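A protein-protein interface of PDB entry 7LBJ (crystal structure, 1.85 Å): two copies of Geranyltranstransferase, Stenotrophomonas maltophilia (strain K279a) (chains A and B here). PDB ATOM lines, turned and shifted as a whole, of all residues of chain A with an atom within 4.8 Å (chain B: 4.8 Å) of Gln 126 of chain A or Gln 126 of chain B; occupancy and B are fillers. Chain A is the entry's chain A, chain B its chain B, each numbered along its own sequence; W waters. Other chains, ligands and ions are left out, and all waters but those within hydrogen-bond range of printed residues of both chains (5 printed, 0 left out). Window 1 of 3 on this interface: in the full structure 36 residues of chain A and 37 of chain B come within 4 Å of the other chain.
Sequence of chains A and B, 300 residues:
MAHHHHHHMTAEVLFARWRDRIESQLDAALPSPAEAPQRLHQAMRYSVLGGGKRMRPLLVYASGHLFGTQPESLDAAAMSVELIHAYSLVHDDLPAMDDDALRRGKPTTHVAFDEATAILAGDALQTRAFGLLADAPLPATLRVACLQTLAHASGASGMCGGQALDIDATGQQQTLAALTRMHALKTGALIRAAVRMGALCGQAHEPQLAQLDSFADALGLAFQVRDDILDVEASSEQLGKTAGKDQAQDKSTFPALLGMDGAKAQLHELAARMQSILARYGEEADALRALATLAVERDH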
ATOM      1  N   ILE A  84      10.493  -5.331 -26.480  1.00  0.00           N
ATOM      2  CA  ILE A  84       9.219  -5.635 -25.831  1.00  0.00           C
ATOM      3  C   ILE A  84       8.083  -4.966 -26.590  1.00  0.00           C
ATOM      4  O   ILE A  84       7.055  -5.585 -26.888  1.00  0.00           O
ATOM      5  CB  ILE A  84       9.245  -5.218 -24.350  1.00  0.00           C
ATOM      6  CG1 ILE A  84      10.247  -6.100 -23.579  1.00  0.00           C
ATOM      7  CG2 ILE A  84       7.844  -5.334 -23.726  1.00  0.00           C
ATOM      8  CD1 ILE A  84       9.932  -7.602 -23.653  1.00  0.00           C
ATOM      9  N   TYR A  87       7.461  -6.829 -30.010  1.00  0.00           N
ATOM     10  CA  TYR A  87       6.802  -8.121 -29.893  1.00  0.00           C
ATOM     11  C   TYR A  87       5.325  -7.924 -29.573  1.00  0.00           C
ATOM     12  O   TYR A  87       4.467  -8.643 -30.096  1.00  0.00           O
ATOM     13  CB  TYR A  87       7.512  -9.014 -28.837  1.00  0.00           C
ATOM     14  CG  TYR A  87       6.713  -9.301 -27.561  1.00  0.00           C
ATOM     15  CD1 TYR A  87       5.559 -10.091 -27.584  1.00  0.00           C
ATOM     16  CD2 TYR A  87       7.123  -8.803 -26.330  1.00  0.00           C
ATOM     17  CE1 TYR A  87       4.804 -10.324 -26.423  1.00  0.00           C
ATOM     18  CE2 TYR A  87       6.379  -9.053 -25.160  1.00  0.00           C
ATOM     19  CZ  TYR A  87       5.234  -9.808 -25.224  1.00  0.00           C
ATOM     20  OH  TYR A  87       4.507 -10.037 -24.085  1.00  0.00           O
ATOM     21  N   GLY A 122       7.162 -13.030 -32.215  1.00  0.00           N
ATOM     22  CA  GLY A 122       6.875 -12.246 -31.023  1.00  0.00           C
ATOM     23  C   GLY A 122       7.469 -12.901 -29.789  1.00  0.00           C
ATOM     24  O   GLY A 122       8.150 -12.255 -28.987  1.00  0.00           O
ATOM     25  N   ASP A 123       7.247 -14.205 -29.642  1.00  0.00           N
ATOM     26  CA  ASP A 123       7.818 -14.923 -28.496  1.00  0.00           C
ATOM     27  C   ASP A 123       9.329 -14.738 -28.426  1.00  0.00           C
ATOM     28  O   ASP A 123       9.885 -14.443 -27.358  1.00  0.00           O
ATOM     29  CB  ASP A 123       7.468 -16.405 -28.584  1.00  0.00           C
ATOM     30  CG  ASP A 123       5.996 -16.672 -28.331  1.00  0.00           C
ATOM     31  OD1 ASP A 123       5.325 -15.772 -27.776  1.00  0.00           O
ATOM     32  OD2 ASP A 123       5.530 -17.794 -28.664  1.00  0.00           O
ATOM     33  N   ALA A 124      10.012 -14.888 -29.566  1.00  0.00           N
ATOM     34  CA  ALA A 124      11.472 -14.831 -29.553  1.00  0.00           C
ATOM     35  C   ALA A 124      11.994 -13.411 -29.358  1.00  0.00           C
ATOM     36  O   ALA A 124      13.108 -13.230 -28.839  1.00  0.00           O
ATOM     37  CB  ALA A 124      12.044 -15.436 -30.846  1.00  0.00           C
ATOM     38  N   LEU A 125      11.256 -12.395 -29.830  1.00  0.00           N
ATOM     39  CA  LEU A 125      11.681 -11.029 -29.562  1.00  0.00           C
ATOM     40  C   LEU A 125      11.598 -10.729 -28.073  1.00  0.00           C
ATOM     41  O   LEU A 125      12.453 -10.014 -27.528  1.00  0.00           O
ATOM     42  CB  LEU A 125      10.834 -10.023 -30.357  1.00  0.00           C
ATOM     43  CG  LEU A 125      11.039 -10.047 -31.873  1.00  0.00           C
ATOM     44  CD1 LEU A 125       9.922  -9.261 -32.573  1.00  0.00           C
ATOM     45  CD2 LEU A 125      12.408  -9.485 -32.231  1.00  0.00           C
ATOM     46  N   GLN A 126      10.559 -11.239 -27.402  1.00  0.00           N
ATOM     47  CA  GLN A 126      10.480 -11.046 -25.955  1.00  0.00           C
ATOM     48  C   GLN A 126      11.698 -11.653 -25.269  1.00  0.00           C
ATOM     49  O   GLN A 126      12.325 -11.011 -24.416  1.00  0.00           O
ATOM     50  CB  GLN A 126       9.195 -11.645 -25.358  1.00  0.00           C
ATOM     51  CG  GLN A 126       9.226 -11.462 -23.829  1.00  0.00           C
ATOM     52  CD  GLN A 126       8.004 -11.993 -23.052  1.00  0.00           C
ATOM     53  OE1 GLN A 126       8.047 -12.043 -21.826  1.00  0.00           O
ATOM     54  NE2 GLN A 126       6.938 -12.385 -23.745  1.00  0.00           N
ATOM     55  N   THR A 127      12.068 -12.883 -25.650  1.00  0.00           N
ATOM     56  CA  THR A 127      13.205 -13.514 -24.993  1.00  0.00           C
ATOM     57  C   THR A 127      14.479 -12.726 -25.253  1.00  0.00           C
ATOM     58  O   THR A 127      15.307 -12.556 -24.350  1.00  0.00           O
ATOM     59  CB  THR A 127      13.374 -14.959 -25.461  1.00  0.00           C
ATOM     60  OG1 THR A 127      12.096 -15.625 -25.460  1.00  0.00           O
ATOM     61  CG2 THR A 127      14.363 -15.702 -24.536  1.00  0.00           C
ATOM     62  N   ARG A 128      14.632 -12.196 -26.476  1.00  0.00           N
ATOM     63  CA  ARG A 128      15.854 -11.471 -26.788  1.00  0.00           C
ATOM     64  C   ARG A 128      15.955 -10.182 -25.989  1.00  0.00           C
ATOM     65  O   ARG A 128      17.067  -9.754 -25.653  1.00  0.00           O
ATOM     66  CB  ARG A 128      15.941 -11.182 -28.295  1.00  0.00           C
ATOM     67  CG  ARG A 128      17.271 -10.575 -28.724  1.00  0.00           C
ATOM     68  CD  ARG A 128      18.423 -11.605 -28.641  1.00  0.00           C
ATOM     69  NE  ARG A 128      19.659 -11.088 -29.244  1.00  0.00           N
ATOM     70  CZ  ARG A 128      20.836 -11.017 -28.626  1.00  0.00           C
ATOM     71  NH1 ARG A 128      20.996 -11.459 -27.386  1.00  0.00           N
ATOM     72  NH2 ARG A 128      21.881 -10.487 -29.271  1.00  0.00           N
ATOM     73  N   ALA A 129      14.822  -9.545 -25.672  1.00  0.00           N
ATOM     74  CA  ALA A 129      14.879  -8.357 -24.824  1.00  0.00           C
ATOM     75  C   ALA A 129      15.521  -8.686 -23.478  1.00  0.00           C
ATOM     76  O   ALA A 129      16.402  -7.960 -23.004  1.00  0.00           O
ATOM     77  CB  ALA A 129      13.477  -7.783 -24.612  1.00  0.00           C
ATOM     78  N   PHE A 130      15.073  -9.766 -22.831  1.00  0.00           N
ATOM     79  CA  PHE A 130      15.665 -10.119 -21.544  1.00  0.00           C
ATOM     80  C   PHE A 130      17.105 -10.593 -21.703  1.00  0.00           C
ATOM     81  O   PHE A 130      17.965 -10.277 -20.870  1.00  0.00           O
ATOM     82  CB  PHE A 130      14.808 -11.179 -20.849  1.00  0.00           C
ATOM     83  CG  PHE A 130      13.473 -10.642 -20.416  1.00  0.00           C
ATOM     84  CD1 PHE A 130      13.396  -9.729 -19.372  1.00  0.00           C
ATOM     85  CD2 PHE A 130      12.308 -11.003 -21.080  1.00  0.00           C
ATOM     86  CE1 PHE A 130      12.164  -9.202 -18.961  1.00  0.00           C
ATOM     87  CE2 PHE A 130      11.054 -10.469 -20.683  1.00  0.00           C
ATOM     88  CZ  PHE A 130      10.996  -9.561 -19.644  1.00  0.00           C
ATOM     89  N   ILE B  84       8.544 -21.257 -18.579  1.00  0.00           N
ATOM     90  CA  ILE B  84       8.872 -21.228 -20.008  1.00  0.00           C
ATOM     91  C   ILE B  84       8.229 -22.420 -20.716  1.00  0.00           C
ATOM     92  O   ILE B  84       7.611 -22.291 -21.781  1.00  0.00           O
ATOM     93  CB  ILE B  84      10.403 -21.220 -20.211  1.00  0.00           C
ATOM     94  CG1 ILE B  84      11.026 -19.935 -19.664  1.00  0.00           C
ATOM     95  CG2 ILE B  84      10.760 -21.387 -21.700  1.00  0.00           C
ATOM     96  CD1 ILE B  84      10.580 -18.632 -20.417  1.00  0.00           C
ATOM     97  N   TYR B  87       4.401 -21.869 -20.991  1.00  0.00           N
ATOM     98  CA  TYR B  87       3.988 -20.906 -22.016  1.00  0.00           C
ATOM     99  C   TYR B  87       4.159 -21.501 -23.406  1.00  0.00           C
ATOM    100  O   TYR B  87       3.317 -21.284 -24.289  1.00  0.00           O
ATOM    101  CB  TYR B  87       4.750 -19.572 -21.874  1.00  0.00           C
ATOM    102  CG  TYR B  87       5.726 -19.236 -23.000  1.00  0.00           C
ATOM    103  CD1 TYR B  87       5.277 -18.841 -24.274  1.00  0.00           C
ATOM    104  CD2 TYR B  87       7.096 -19.266 -22.781  1.00  0.00           C
ATOM    105  CE1 TYR B  87       6.174 -18.552 -25.297  1.00  0.00           C
ATOM    106  CE2 TYR B  87       8.005 -18.947 -23.798  1.00  0.00           C
ATOM    107  CZ  TYR B  87       7.539 -18.608 -25.051  1.00  0.00           C
ATOM    108  OH  TYR B  87       8.449 -18.311 -26.039  1.00  0.00           O
ATOM    109  N   GLY B 122       0.250 -16.982 -22.431  1.00  0.00           N
ATOM    110  CA  GLY B 122       1.591 -17.439 -22.765  1.00  0.00           C
ATOM    111  C   GLY B 122       2.617 -16.327 -22.643  1.00  0.00           C
ATOM    112  O   GLY B 122       3.678 -16.503 -22.033  1.00  0.00           O
ATOM    113  N   ASP B 123       2.296 -15.153 -23.196  1.00  0.00           N
ATOM    114  CA  ASP B 123       3.216 -14.015 -23.144  1.00  0.00           C
ATOM    115  C   ASP B 123       3.538 -13.651 -21.706  1.00  0.00           C
ATOM    116  O   ASP B 123       4.702 -13.401 -21.359  1.00  0.00           O
ATOM    117  CB  ASP B 123       2.603 -12.806 -23.858  1.00  0.00           C
ATOM    118  CG  ASP B 123       2.529 -12.974 -25.376  1.00  0.00           C
ATOM    119  OD1 ASP B 123       3.218 -13.869 -25.913  1.00  0.00           O
ATOM    120  OD2 ASP B 123       1.801 -12.176 -26.041  1.00  0.00           O
ATOM    121  N   ALA B 124       2.521 -13.650 -20.846  1.00  0.00           N
ATOM    122  CA  ALA B 124       2.721 -13.220 -19.469  1.00  0.00           C
ATOM    123  C   ALA B 124       3.462 -14.262 -18.648  1.00  0.00           C
ATOM    124  O   ALA B 124       4.209 -13.893 -17.733  1.00  0.00           O
ATOM    125  CB  ALA B 124       1.376 -12.895 -18.817  1.00  0.00           C
ATOM    126  N   LEU B 125       3.249 -15.558 -18.931  1.00  0.00           N
ATOM    127  CA  LEU B 125       4.032 -16.594 -18.251  1.00  0.00           C
ATOM    128  C   LEU B 125       5.510 -16.490 -18.611  1.00  0.00           C
ATOM    129  O   LEU B 125       6.375 -16.695 -17.748  1.00  0.00           O
ATOM    130  CB  LEU B 125       3.511 -17.991 -18.594  1.00  0.00           C
ATOM    131  CG  LEU B 125       2.111 -18.312 -18.045  1.00  0.00           C
ATOM    132  CD1 LEU B 125       1.582 -19.556 -18.711  1.00  0.00           C
ATOM    133  CD2 LEU B 125       2.144 -18.511 -16.528  1.00  0.00           C
ATOM    134  N   GLN B 126       5.823 -16.204 -19.881  1.00  0.00           N
ATOM    135  CA  GLN B 126       7.229 -15.995 -20.231  1.00  0.00           C
ATOM    136  C   GLN B 126       7.820 -14.854 -19.412  1.00  0.00           C
ATOM    137  O   GLN B 126       8.904 -14.988 -18.838  1.00  0.00           O
ATOM    138  CB  GLN B 126       7.426 -15.714 -21.731  1.00  0.00           C
ATOM    139  CG  GLN B 126       8.960 -15.532 -21.988  1.00  0.00           C
ATOM    140  CD  GLN B 126       9.432 -15.219 -23.430  1.00  0.00           C
ATOM    141  OE1 GLN B 126      10.634 -15.016 -23.639  1.00  0.00           O
ATOM    142  NE2 GLN B 126       8.534 -15.215 -24.403  1.00  0.00           N
ATOM    143  N   THR B 127       7.123 -13.712 -19.345  1.00  0.00           N
ATOM    144  CA  THR B 127       7.652 -12.605 -18.563  1.00  0.00           C
ATOM    145  C   THR B 127       7.821 -12.990 -17.094  1.00  0.00           C
ATOM    146  O   THR B 127       8.808 -12.614 -16.456  1.00  0.00           O
ATOM    147  CB  THR B 127       6.735 -11.392 -18.668  1.00  0.00           C
ATOM    148  OG1 THR B 127       6.570 -11.058 -20.059  1.00  0.00           O
ATOM    149  CG2 THR B 127       7.384 -10.212 -17.975  1.00  0.00           C
ATOM    150  N   ARG B 128       6.842 -13.688 -16.532  1.00  0.00           N
ATOM    151  CA  ARG B 128       6.927 -14.028 -15.112  1.00  0.00           C
ATOM    152  C   ARG B 128       8.144 -14.910 -14.833  1.00  0.00           C
ATOM    153  O   ARG B 128       8.769 -14.815 -13.760  1.00  0.00           O
ATOM    154  CB  ARG B 128       5.642 -14.734 -14.670  1.00  0.00           C
ATOM    155  CG  ARG B 128       5.512 -14.928 -13.156  1.00  0.00           C
ATOM    156  CD  ARG B 128       5.724 -13.612 -12.386  1.00  0.00           C
ATOM    157  NE  ARG B 128       5.450 -13.811 -10.969  1.00  0.00           N
ATOM    158  CZ  ARG B 128       6.133 -13.251  -9.979  1.00  0.00           C
ATOM    159  NH1 ARG B 128       7.167 -12.453 -10.213  1.00  0.00           N
ATOM    160  NH2 ARG B 128       5.777 -13.513  -8.717  1.00  0.00           N
ATOM    161  N   ALA B 129       8.473 -15.797 -15.770  1.00  0.00           N
ATOM    162  CA  ALA B 129       9.652 -16.646 -15.584  1.00  0.00           C
ATOM    163  C   ALA B 129      10.901 -15.800 -15.394  1.00  0.00           C
ATOM    164  O   ALA B 129      11.687 -16.033 -14.469  1.00  0.00           O
ATOM    165  CB  ALA B 129       9.825 -17.582 -16.778  1.00  0.00           C
ATOM    166  N   PHE B 130      11.085 -14.782 -16.249  1.00  0.00           N
ATOM    167  CA  PHE B 130      12.243 -13.904 -16.100  1.00  0.00           C
ATOM    168  C   PHE B 130      12.150 -13.037 -14.840  1.00  0.00           C
ATOM    169  O   PHE B 130      13.158 -12.821 -14.150  1.00  0.00           O
ATOM    170  CB  PHE B 130      12.408 -13.058 -17.374  1.00  0.00           C
ATOM    171  CG  PHE B 130      12.931 -13.865 -18.529  1.00  0.00           C
ATOM    172  CD1 PHE B 130      14.256 -14.285 -18.543  1.00  0.00           C
ATOM    173  CD2 PHE B 130      12.086 -14.277 -19.555  1.00  0.00           C
ATOM    174  CE1 PHE B 130      14.748 -15.083 -19.581  1.00  0.00           C
ATOM    175  CE2 PHE B 130      12.568 -15.065 -20.620  1.00  0.00           C
ATOM    176  CZ  PHE B 130      13.905 -15.472 -20.624  1.00  0.00           C
HETATM  177  O   HOH W   1       1.724  -9.236 -25.452  1.00  0.00           O
HETATM  178  O   HOH W   2       5.898 -15.274 -24.880  1.00  0.00           O
HETATM  179  O   HOH W   3       5.508  -9.351 -21.928  1.00  0.00           O
HETATM  180  O   HOH W   4      11.014 -18.054 -25.347  1.00  0.00           O
HETATM  181  O   HOH W   5       7.131 -20.410 -27.839  1.00  0.00           O
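The side-chain amide nitrogen (NE2) of Gln 126 of chain B sits at hydrogen-bond distance from the backbone carbonyl oxygen (O) of Asp 123 of chain A (3.3 Å). NE2 of Gln 126 of chain A lies within hydrogen-bond range of O of Asp 123 of chain B (3.4 Å). The side-chain amide nitrogen (NE2) of Gln 126 of chain B lies close to the side-chain amide nitrogen (NE2) of Gln 126 of chain A (3.3 Å). The side-chain amide oxygen (OE1) of Gln 126 of chain A lies within hydrogen-bond range of the side-chain hydroxyl (OG1) of Thr 127 of chain B (2.5 Å). The side-chain hydroxyl (OG1) of Thr 127 of chain A lies within hydrogen-bond range of the side-chain amide oxygen (OE1) of Gln 126 of chain B (2.4 Å). OD1 of Asp 123 of chain A sits close to OD1 of Asp 123 of chain B (3.4 Å).
The side-chain hydroxyl of Tyr 87 of chain A is in hydrogen-bond range of the side-chain amide nitrogen of Gln 126 of chain A (3.4 Å). O of Asp 123 of chain A lies within hydrogen-bond range of OG1 of Thr 127 of chain A (3.1 Å). The backbone carbonyl oxygen of Asp 123 of chain B is in hydrogen-bond range of the side-chain hydroxyl of Thr 127 of chain B, 3.3 Å away.
Among the printed residues, pairs that only touch across the chains: Asp 123 of chain A with Tyr 87 of chain B (3.3 Å), Tyr 87 of chain A with Asp 123 of chain B (3.4 Å), Phe 130 of chain A with Phe 130 of chain B (3.6 Å) and Thr 127 of chain A with Phe 130 of chain B (3.9 Å).
Of the printed residues of chain B, Asp 123 of chain A touches Tyr 87, Asp 123 and Gln 126. Printed residues of chain A within 4 Å of Tyr 87 of chain B: Asp 123 (3.3 Å). Of the printed residues of chain A, Asp 123 of chain B touches Tyr 87 (3.4 Å), Asp 123 (3.4 Å) and Gln 126 (3.4 Å). Gln 126 of chain B touches three residues of chain A. Of the printed residues of chain A, Phe 130 of chain B touches Thr 127 and Phe 130. The nearest printed residue of chain B that does not touch Gln 126 of chain A is Phe 130 of chain B (5.1 Å). The nearest printed residue of chain A that does not touch Gln 126 of chain B is Phe 130 of chain A (5.0 Å). The nearest printed residue of chain B that does not touch Tyr 87 of chain A is Thr 127 of chain B (4.6 Å).
Printed residues of chain B that touch a printed residue of chain A: Tyr 87, Asp 123, Gln 126, Thr 127 and Phe 130. Hydrophobic or aromatic side chains of chain B that line the printed part of chain A: Tyr 87 and Phe 130. Hydrophobic or aromatic side chains of chain A that line the printed part of chain B: Tyr 87 and Phe 130. Among the printed residues, 10 pairs touch across the chains.
Tyr 87 of chain A touches Asp 123 of chain B, and with the chains exchanged Asp 123 of chain A touches Tyr 87 of chain B. Asp 123 of chain A touches its own counterpart, Asp 123 of chain B. Gln 126 of chain A touches Thr 127 of chain B, and with the chains exchanged Thr 127 of chain A touches Gln 126 of chain B. Thr 127 of chain A touches Phe 130 of chain B, but with the chains exchanged Phe 130 of chain A does not touch Thr 127 of chain B (4.03 Å). 11 positions are printed for both chains. Of the 10 pairs that touch across the chains among the printed residues, 9 have their exchanged pair printed and touching as well.
Water W3 bridges OH of Tyr 87 of chain A (2.5 Å) and OG1 of Thr 127 of chain B (2.7 Å). Water W4 lies within hydrogen-bond range of the side-chain hydroxyl of Thr 127 of chain A (2.7 Å) and the side-chain hydroxyl of Tyr 87 of chain B (2.7 Å). Water W2 lies within hydrogen-bond range of NE2 of Gln 126 of chain B, OD1 of Asp 123 of chain A, OD1 of Asp 123 of chain B and NE2 of Gln 126 of chain A. Water W1 bridges the side-chain carboxylate of Asp 123 of chain B (3.0 Å) and the side-chain hydroxyl of Tyr 87 of chain A (3.2 Å). Water W5 lies within hydrogen-bond range of OH of Tyr 87 of chain B (3.1 Å) and OD2 of Asp 123 of chain A (3.2 Å).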
